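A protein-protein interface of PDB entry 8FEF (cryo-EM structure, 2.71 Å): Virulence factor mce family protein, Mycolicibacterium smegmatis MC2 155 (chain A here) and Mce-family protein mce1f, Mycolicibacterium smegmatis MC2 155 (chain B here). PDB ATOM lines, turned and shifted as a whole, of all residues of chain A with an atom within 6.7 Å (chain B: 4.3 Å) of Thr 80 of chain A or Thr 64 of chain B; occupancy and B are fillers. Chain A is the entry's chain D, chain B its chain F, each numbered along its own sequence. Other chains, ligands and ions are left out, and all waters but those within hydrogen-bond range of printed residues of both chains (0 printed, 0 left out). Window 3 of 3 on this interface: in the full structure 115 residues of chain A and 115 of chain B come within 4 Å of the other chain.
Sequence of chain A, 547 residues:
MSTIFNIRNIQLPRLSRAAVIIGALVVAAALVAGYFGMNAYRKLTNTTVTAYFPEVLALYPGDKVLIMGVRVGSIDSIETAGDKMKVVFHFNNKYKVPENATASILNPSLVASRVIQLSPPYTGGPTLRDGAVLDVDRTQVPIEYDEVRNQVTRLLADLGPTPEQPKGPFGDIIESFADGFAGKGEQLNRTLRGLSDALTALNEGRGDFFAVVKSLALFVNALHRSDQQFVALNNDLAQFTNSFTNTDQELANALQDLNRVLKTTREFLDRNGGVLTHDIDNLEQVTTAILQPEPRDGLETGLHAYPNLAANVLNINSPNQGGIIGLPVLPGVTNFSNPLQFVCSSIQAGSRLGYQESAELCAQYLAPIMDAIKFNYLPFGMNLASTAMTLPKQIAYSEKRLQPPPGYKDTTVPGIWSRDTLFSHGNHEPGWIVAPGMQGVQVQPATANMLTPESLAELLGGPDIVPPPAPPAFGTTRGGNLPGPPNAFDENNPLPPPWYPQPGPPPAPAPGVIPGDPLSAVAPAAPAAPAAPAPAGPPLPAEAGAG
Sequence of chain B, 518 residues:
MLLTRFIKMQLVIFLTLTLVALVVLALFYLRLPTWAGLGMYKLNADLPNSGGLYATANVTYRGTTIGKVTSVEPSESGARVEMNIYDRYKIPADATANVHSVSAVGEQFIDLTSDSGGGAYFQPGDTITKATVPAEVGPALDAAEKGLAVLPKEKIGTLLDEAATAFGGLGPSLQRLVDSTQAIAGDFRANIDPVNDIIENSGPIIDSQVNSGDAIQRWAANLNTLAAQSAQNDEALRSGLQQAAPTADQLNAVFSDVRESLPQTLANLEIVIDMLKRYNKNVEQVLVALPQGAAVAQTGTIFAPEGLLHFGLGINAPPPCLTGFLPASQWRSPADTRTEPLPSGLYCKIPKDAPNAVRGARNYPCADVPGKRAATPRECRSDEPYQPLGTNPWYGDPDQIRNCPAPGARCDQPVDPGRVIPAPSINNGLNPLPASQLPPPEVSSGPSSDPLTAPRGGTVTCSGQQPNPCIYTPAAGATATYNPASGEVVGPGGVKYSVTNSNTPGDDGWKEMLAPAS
Of chain A, only Val 56 (3.7 Å), Thr 80 (3.97 Å) and Met 85 (3.6 Å) come within 4 Å of Thr 64 of chain B.
Of the printed residues of chain B, Asp 83 of chain A touches Arg 62.
Printed residues of chain A within 4 Å of Tyr 61 of chain B: Thr 80 (3.5 Å) and Gly 82 (3.5 Å).
Ile 78 of chain A touches none of the printed residues of chain B.
Leu 59 of chain A touches none of the printed residues of chain B.
The nearest printed residue of chain B that does not touch Thr 80 of chain A is Ile 66 of chain B (5.5 Å).
The nearest residue of chain A that does not touch Thr 64 of chain B is Ile 78 of chain A (4.5 Å).
OG1 of Thr 80 of chain A sits close to SD of Met 85 of chain A (3.8 Å).
Val 56 of chain A touches Thr 64 of chain B.
Thr 80 of chain A touches Tyr 61 of chain B.
OG1 of Thr 80 of chain A touches CG2 of Thr 64 of chain B, at 3.97 Å.
Tyr 61 of chain B touches Gly 82 of chain A (OH to O, 3.5 Å).
Met 85 of chain A touches Arg 62 of chain B (SD to CB, 3.7 Å).
CG2 of Thr 64 of chain B touches CE of Met 85 of chain A, 3.6 Å away.
O of Asp 83 of chain A sits at hydrogen-bond distance from NE of Arg 62 of chain B.
The backbone carbonyl oxygen (O) of Val 56 of chain A lies close to the backbone carbonyl oxygen (O) of Gly 63 of chain B (3.4 Å).
The backbone NH of Val 56 of chain A is in hydrogen-bond range of the backbone carbonyl oxygen of Arg 62 of chain B.
Of the 8 printed residues of chain B, 4 touch a printed residue of chain A.
Of the 13 printed residues of chain A, 5 touch a printed residue of chain B.
Hydrophobic or aromatic side chains of chain A that line the printed part of chain B: Met 85.
Among the printed residues, 9 pairs touch across the chains.
Among the printed residues, no Asp or Glu carboxylate lies within 4 Å of a Lys or Arg side-chain nitrogen of the other chain.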
ATOM      1  N   VAL A  56      11.008  28.175 -11.253  1.00  0.00           N
ATOM      2  CA  VAL A  56      12.172  28.378 -12.115  1.00  0.00           C
ATOM      3  C   VAL A  56      11.645  28.981 -13.415  1.00  0.00           C
ATOM      4  O   VAL A  56      11.200  28.266 -14.317  1.00  0.00           O
ATOM      5  CB  VAL A  56      12.951  27.084 -12.369  1.00  0.00           C
ATOM      6  CG1 VAL A  56      14.024  27.296 -13.412  1.00  0.00           C
ATOM      7  CG2 VAL A  56      13.589  26.599 -11.084  1.00  0.00           C
ATOM      8  N   LEU A  57      11.679  30.306 -13.511  1.00  0.00           N
ATOM      9  CA  LEU A  57      11.161  31.033 -14.660  1.00  0.00           C
ATOM     10  C   LEU A  57      12.307  31.684 -15.422  1.00  0.00           C
ATOM     11  O   LEU A  57      13.229  32.237 -14.817  1.00  0.00           O
ATOM     12  CB  LEU A  57      10.151  32.098 -14.228  1.00  0.00           C
ATOM     13  CG  LEU A  57       9.682  33.072 -15.311  1.00  0.00           C
ATOM     14  CD1 LEU A  57       8.974  32.326 -16.426  1.00  0.00           C
ATOM     15  CD2 LEU A  57       8.784  34.149 -14.730  1.00  0.00           C
ATOM     16  N   ALA A  58      12.242  31.598 -16.753  1.00  0.00           N
ATOM     17  CA  ALA A  58      13.222  32.182 -17.669  1.00  0.00           C
ATOM     18  C   ALA A  58      14.636  31.677 -17.411  1.00  0.00           C
ATOM     19  O   ALA A  58      15.614  32.340 -17.770  1.00  0.00           O
ATOM     20  CB  ALA A  58      13.190  33.714 -17.626  1.00  0.00           C
ATOM     21  N   LEU A  59      14.760  30.511 -16.790  1.00  0.00           N
ATOM     22  CA  LEU A  59      16.037  29.853 -16.565  1.00  0.00           C
ATOM     23  C   LEU A  59      16.060  28.577 -17.391  1.00  0.00           C
ATOM     24  O   LEU A  59      15.145  27.753 -17.291  1.00  0.00           O
ATOM     25  CB  LEU A  59      16.240  29.542 -15.083  1.00  0.00           C
ATOM     26  CG  LEU A  59      17.639  29.126 -14.638  1.00  0.00           C
ATOM     27  CD1 LEU A  59      18.553  30.334 -14.608  1.00  0.00           C
ATOM     28  CD2 LEU A  59      17.592  28.447 -13.284  1.00  0.00           C
ATOM     29  N   ILE A  78      16.862  21.008 -15.886  1.00  0.00           N
ATOM     30  CA  ILE A  78      15.770  21.518 -15.059  1.00  0.00           C
ATOM     31  C   ILE A  78      14.560  20.622 -15.287  1.00  0.00           C
ATOM     32  O   ILE A  78      14.040  20.558 -16.405  1.00  0.00           O
ATOM     33  CB  ILE A  78      15.412  22.978 -15.392  1.00  0.00           C
ATOM     34  CG1 ILE A  78      16.603  23.904 -15.143  1.00  0.00           C
ATOM     35  CG2 ILE A  78      14.205  23.428 -14.587  1.00  0.00           C
ATOM     36  CD1 ILE A  78      16.362  25.325 -15.562  1.00  0.00           C
ATOM     37  N   GLU A  79      14.106  19.935 -14.238  1.00  0.00           N
ATOM     38  CA  GLU A  79      12.945  19.064 -14.358  1.00  0.00           C
ATOM     39  C   GLU A  79      12.024  19.235 -13.158  1.00  0.00           C
ATOM     40  O   GLU A  79      12.468  19.540 -12.051  1.00  0.00           O
ATOM     41  CB  GLU A  79      13.353  17.587 -14.497  1.00  0.00           C
ATOM     42  CG  GLU A  79      14.071  16.998 -13.291  1.00  0.00           C
ATOM     43  CD  GLU A  79      15.573  17.213 -13.331  1.00  0.00           C
ATOM     44  OE1 GLU A  79      16.039  18.070 -14.111  1.00  0.00           O
ATOM     45  OE2 GLU A  79      16.290  16.520 -12.579  1.00  0.00           O
ATOM     46  N   THR A  80      10.730  19.032 -13.391  1.00  0.00           N
ATOM     47  CA  THR A  80       9.746  19.132 -12.322  1.00  0.00           C
ATOM     48  C   THR A  80       9.926  17.996 -11.320  1.00  0.00           C
ATOM     49  O   THR A  80      10.130  16.841 -11.702  1.00  0.00           O
ATOM     50  CB  THR A  80       8.333  19.095 -12.905  1.00  0.00           C
ATOM     51  OG1 THR A  80       8.180  20.150 -13.862  1.00  0.00           O
ATOM     52  CG2 THR A  80       7.293  19.257 -11.810  1.00  0.00           C
ATOM     53  N   ALA A  81       9.849  18.326 -10.028  1.00  0.00           N
ATOM     54  CA  ALA A  81       9.907  17.344  -8.947  1.00  0.00           C
ATOM     55  C   ALA A  81       8.739  17.644  -8.011  1.00  0.00           C
ATOM     56  O   ALA A  81       8.885  18.406  -7.051  1.00  0.00           O
ATOM     57  CB  ALA A  81      11.246  17.393  -8.221  1.00  0.00           C
ATOM     58  N   GLY A  82       7.589  17.045  -8.296  1.00  0.00           N
ATOM     59  CA  GLY A  82       6.400  17.307  -7.502  1.00  0.00           C
ATOM     60  C   GLY A  82       5.986  18.760  -7.622  1.00  0.00           C
ATOM     61  O   GLY A  82       5.768  19.281  -8.722  1.00  0.00           O
ATOM     62  N   ASP A  83       5.869  19.430  -6.480  1.00  0.00           N
ATOM     63  CA  ASP A  83       5.549  20.849  -6.439  1.00  0.00           C
ATOM     64  C   ASP A  83       6.788  21.733  -6.485  1.00  0.00           C
ATOM     65  O   ASP A  83       6.663  22.957  -6.377  1.00  0.00           O
ATOM     66  CB  ASP A  83       4.732  21.172  -5.185  1.00  0.00           C
ATOM     67  CG  ASP A  83       5.416  20.719  -3.912  1.00  0.00           C
ATOM     68  OD1 ASP A  83       6.152  19.712  -3.959  1.00  0.00           O
ATOM     69  OD2 ASP A  83       5.216  21.368  -2.865  1.00  0.00           O
ATOM     70  N   LYS A  84       7.975  21.150  -6.630  1.00  0.00           N
ATOM     71  CA  LYS A  84       9.219  21.896  -6.714  1.00  0.00           C
ATOM     72  C   LYS A  84       9.825  21.741  -8.106  1.00  0.00           C
ATOM     73  O   LYS A  84       9.343  20.976  -8.947  1.00  0.00           O
ATOM     74  CB  LYS A  84      10.200  21.426  -5.638  1.00  0.00           C
ATOM     75  CG  LYS A  84       9.619  21.388  -4.241  1.00  0.00           C
ATOM     76  CD  LYS A  84      10.593  20.750  -3.266  1.00  0.00           C
ATOM     77  CE  LYS A  84      10.013  20.690  -1.864  1.00  0.00           C
ATOM     78  NZ  LYS A  84      10.957  20.059  -0.902  1.00  0.00           N
ATOM     79  N   MET A  85      10.916  22.464  -8.340  1.00  0.00           N
ATOM     80  CA  MET A  85      11.684  22.348  -9.570  1.00  0.00           C
ATOM     81  C   MET A  85      13.113  21.967  -9.216  1.00  0.00           C
ATOM     82  O   MET A  85      13.774  22.678  -8.452  1.00  0.00           O
ATOM     83  CB  MET A  85      11.651  23.655 -10.360  1.00  0.00           C
ATOM     84  CG  MET A  85      10.254  24.153 -10.669  1.00  0.00           C
ATOM     85  SD  MET A  85       9.313  22.956 -11.625  1.00  0.00           S
ATOM     86  CE  MET A  85      10.421  22.711 -13.006  1.00  0.00           C
ATOM     87  N   LYS A  86      13.573  20.844  -9.758  1.00  0.00           N
ATOM     88  CA  LYS A  86      14.908  20.325  -9.512  1.00  0.00           C
ATOM     89  C   LYS A  86      15.830  20.809 -10.624  1.00  0.00           C
ATOM     90  O   LYS A  86      15.625  20.475 -11.797  1.00  0.00           O
ATOM     91  CB  LYS A  86      14.867  18.799  -9.451  1.00  0.00           C
ATOM     92  CG  LYS A  86      16.209  18.103  -9.446  1.00  0.00           C
ATOM     93  CD  LYS A  86      16.011  16.610  -9.224  1.00  0.00           C
ATOM     94  CE  LYS A  86      17.318  15.845  -9.285  1.00  0.00           C
ATOM     95  NZ  LYS A  86      17.860  15.796 -10.668  1.00  0.00           N
ATOM     96  N   VAL B  59       3.394  27.470 -22.877  1.00  0.00           N
ATOM     97  CA  VAL B  59       2.720  26.896 -21.723  1.00  0.00           C
ATOM     98  C   VAL B  59       3.798  26.363 -20.797  1.00  0.00           C
ATOM     99  O   VAL B  59       4.687  25.624 -21.232  1.00  0.00           O
ATOM    100  CB  VAL B  59       1.748  25.777 -22.133  1.00  0.00           C
ATOM    101  CG1 VAL B  59       1.064  25.197 -20.910  1.00  0.00           C
ATOM    102  CG2 VAL B  59       0.730  26.297 -23.120  1.00  0.00           C
ATOM    103  N   THR B  60       3.743  26.755 -19.530  1.00  0.00           N
ATOM    104  CA  THR B  60       4.771  26.406 -18.570  1.00  0.00           C
ATOM    105  C   THR B  60       4.138  25.781 -17.337  1.00  0.00           C
ATOM    106  O   THR B  60       2.960  25.980 -17.046  1.00  0.00           O
ATOM    107  CB  THR B  60       5.598  27.632 -18.153  1.00  0.00           C
ATOM    108  OG1 THR B  60       4.742  28.602 -17.539  1.00  0.00           O
ATOM    109  CG2 THR B  60       6.282  28.260 -19.359  1.00  0.00           C
ATOM    110  N   TYR B  61       4.941  24.987 -16.641  1.00  0.00           N
ATOM    111  CA  TYR B  61       4.641  24.513 -15.298  1.00  0.00           C
ATOM    112  C   TYR B  61       5.717  25.077 -14.385  1.00  0.00           C
ATOM    113  O   TYR B  61       6.901  24.761 -14.554  1.00  0.00           O
ATOM    114  CB  TYR B  61       4.605  22.984 -15.233  1.00  0.00           C
ATOM    115  CG  TYR B  61       4.182  22.442 -13.886  1.00  0.00           C
ATOM    116  CD1 TYR B  61       5.116  22.191 -12.890  1.00  0.00           C
ATOM    117  CD2 TYR B  61       2.847  22.182 -13.611  1.00  0.00           C
ATOM    118  CE1 TYR B  61       4.730  21.700 -11.658  1.00  0.00           C
ATOM    119  CE2 TYR B  61       2.453  21.689 -12.382  1.00  0.00           C
ATOM    120  CZ  TYR B  61       3.400  21.450 -11.411  1.00  0.00           C
ATOM    121  OH  TYR B  61       3.015  20.960 -10.184  1.00  0.00           O
ATOM    122  N   ARG B  62       5.308  25.938 -13.450  1.00  0.00           N
ATOM    123  CA  ARG B  62       6.220  26.602 -12.512  1.00  0.00           C
ATOM    124  C   ARG B  62       7.400  27.255 -13.230  1.00  0.00           C
ATOM    125  O   ARG B  62       8.499  27.362 -12.683  1.00  0.00           O
ATOM    126  CB  ARG B  62       6.708  25.631 -11.436  1.00  0.00           C
ATOM    127  CG  ARG B  62       5.610  25.174 -10.496  1.00  0.00           C
ATOM    128  CD  ARG B  62       6.175  24.499  -9.263  1.00  0.00           C
ATOM    129  NE  ARG B  62       5.132  24.196  -8.291  1.00  0.00           N
ATOM    130  CZ  ARG B  62       4.666  25.060  -7.400  1.00  0.00           C
ATOM    131  NH1 ARG B  62       5.133  26.295  -7.324  1.00  0.00           N
ATOM    132  NH2 ARG B  62       3.708  24.674  -6.562  1.00  0.00           N
ATOM    133  N   GLY B  63       7.172  27.698 -14.466  1.00  0.00           N
ATOM    134  CA  GLY B  63       8.151  28.415 -15.241  1.00  0.00           C
ATOM    135  C   GLY B  63       8.836  27.610 -16.328  1.00  0.00           C
ATOM    136  O   GLY B  63       9.438  28.212 -17.225  1.00  0.00           O
ATOM    137  N   THR B  64       8.768  26.278 -16.289  1.00  0.00           N
ATOM    138  CA  THR B  64       9.452  25.475 -17.299  1.00  0.00           C
ATOM    139  C   THR B  64       8.489  25.128 -18.430  1.00  0.00           C
ATOM    140  O   THR B  64       7.317  24.830 -18.196  1.00  0.00           O
ATOM    141  CB  THR B  64      10.068  24.205 -16.693  1.00  0.00           C
ATOM    142  OG1 THR B  64      10.951  23.602 -17.647  1.00  0.00           O
ATOM    143  CG2 THR B  64       9.016  23.180 -16.295  1.00  0.00           C
ATOM    144  N   THR B  65       8.975  25.217 -19.665  1.00  0.00           N
ATOM    145  CA  THR B  65       8.104  25.022 -20.819  1.00  0.00           C
ATOM    146  C   THR B  65       7.697  23.558 -20.941  1.00  0.00           C
ATOM    147  O   THR B  65       8.545  22.661 -20.908  1.00  0.00           O
ATOM    148  CB  THR B  65       8.802  25.488 -22.095  1.00  0.00           C
ATOM    149  OG1 THR B  65       9.102  26.885 -21.992  1.00  0.00           O
ATOM    150  CG2 THR B  65       7.912  25.258 -23.305  1.00  0.00           C
ATOM    151  N   ILE B  66       6.392  23.318 -21.077  1.00  0.00           N
ATOM    152  CA  ILE B  66       5.841  21.972 -21.190  1.00  0.00           C
ATOM    153  C   ILE B  66       4.885  21.909 -22.374  1.00  0.00           C
ATOM    154  O   ILE B  66       4.215  20.893 -22.588  1.00  0.00           O
ATOM    155  CB  ILE B  66       5.119  21.545 -19.897  1.00  0.00           C
ATOM    156  CG1 ILE B  66       3.836  22.357 -19.709  1.00  0.00           C
ATOM    157  CG2 ILE B  66       6.030  21.682 -18.683  1.00  0.00           C
ATOM    158  CD1 ILE B  66       2.959  21.854 -18.590  1.00  0.00           C
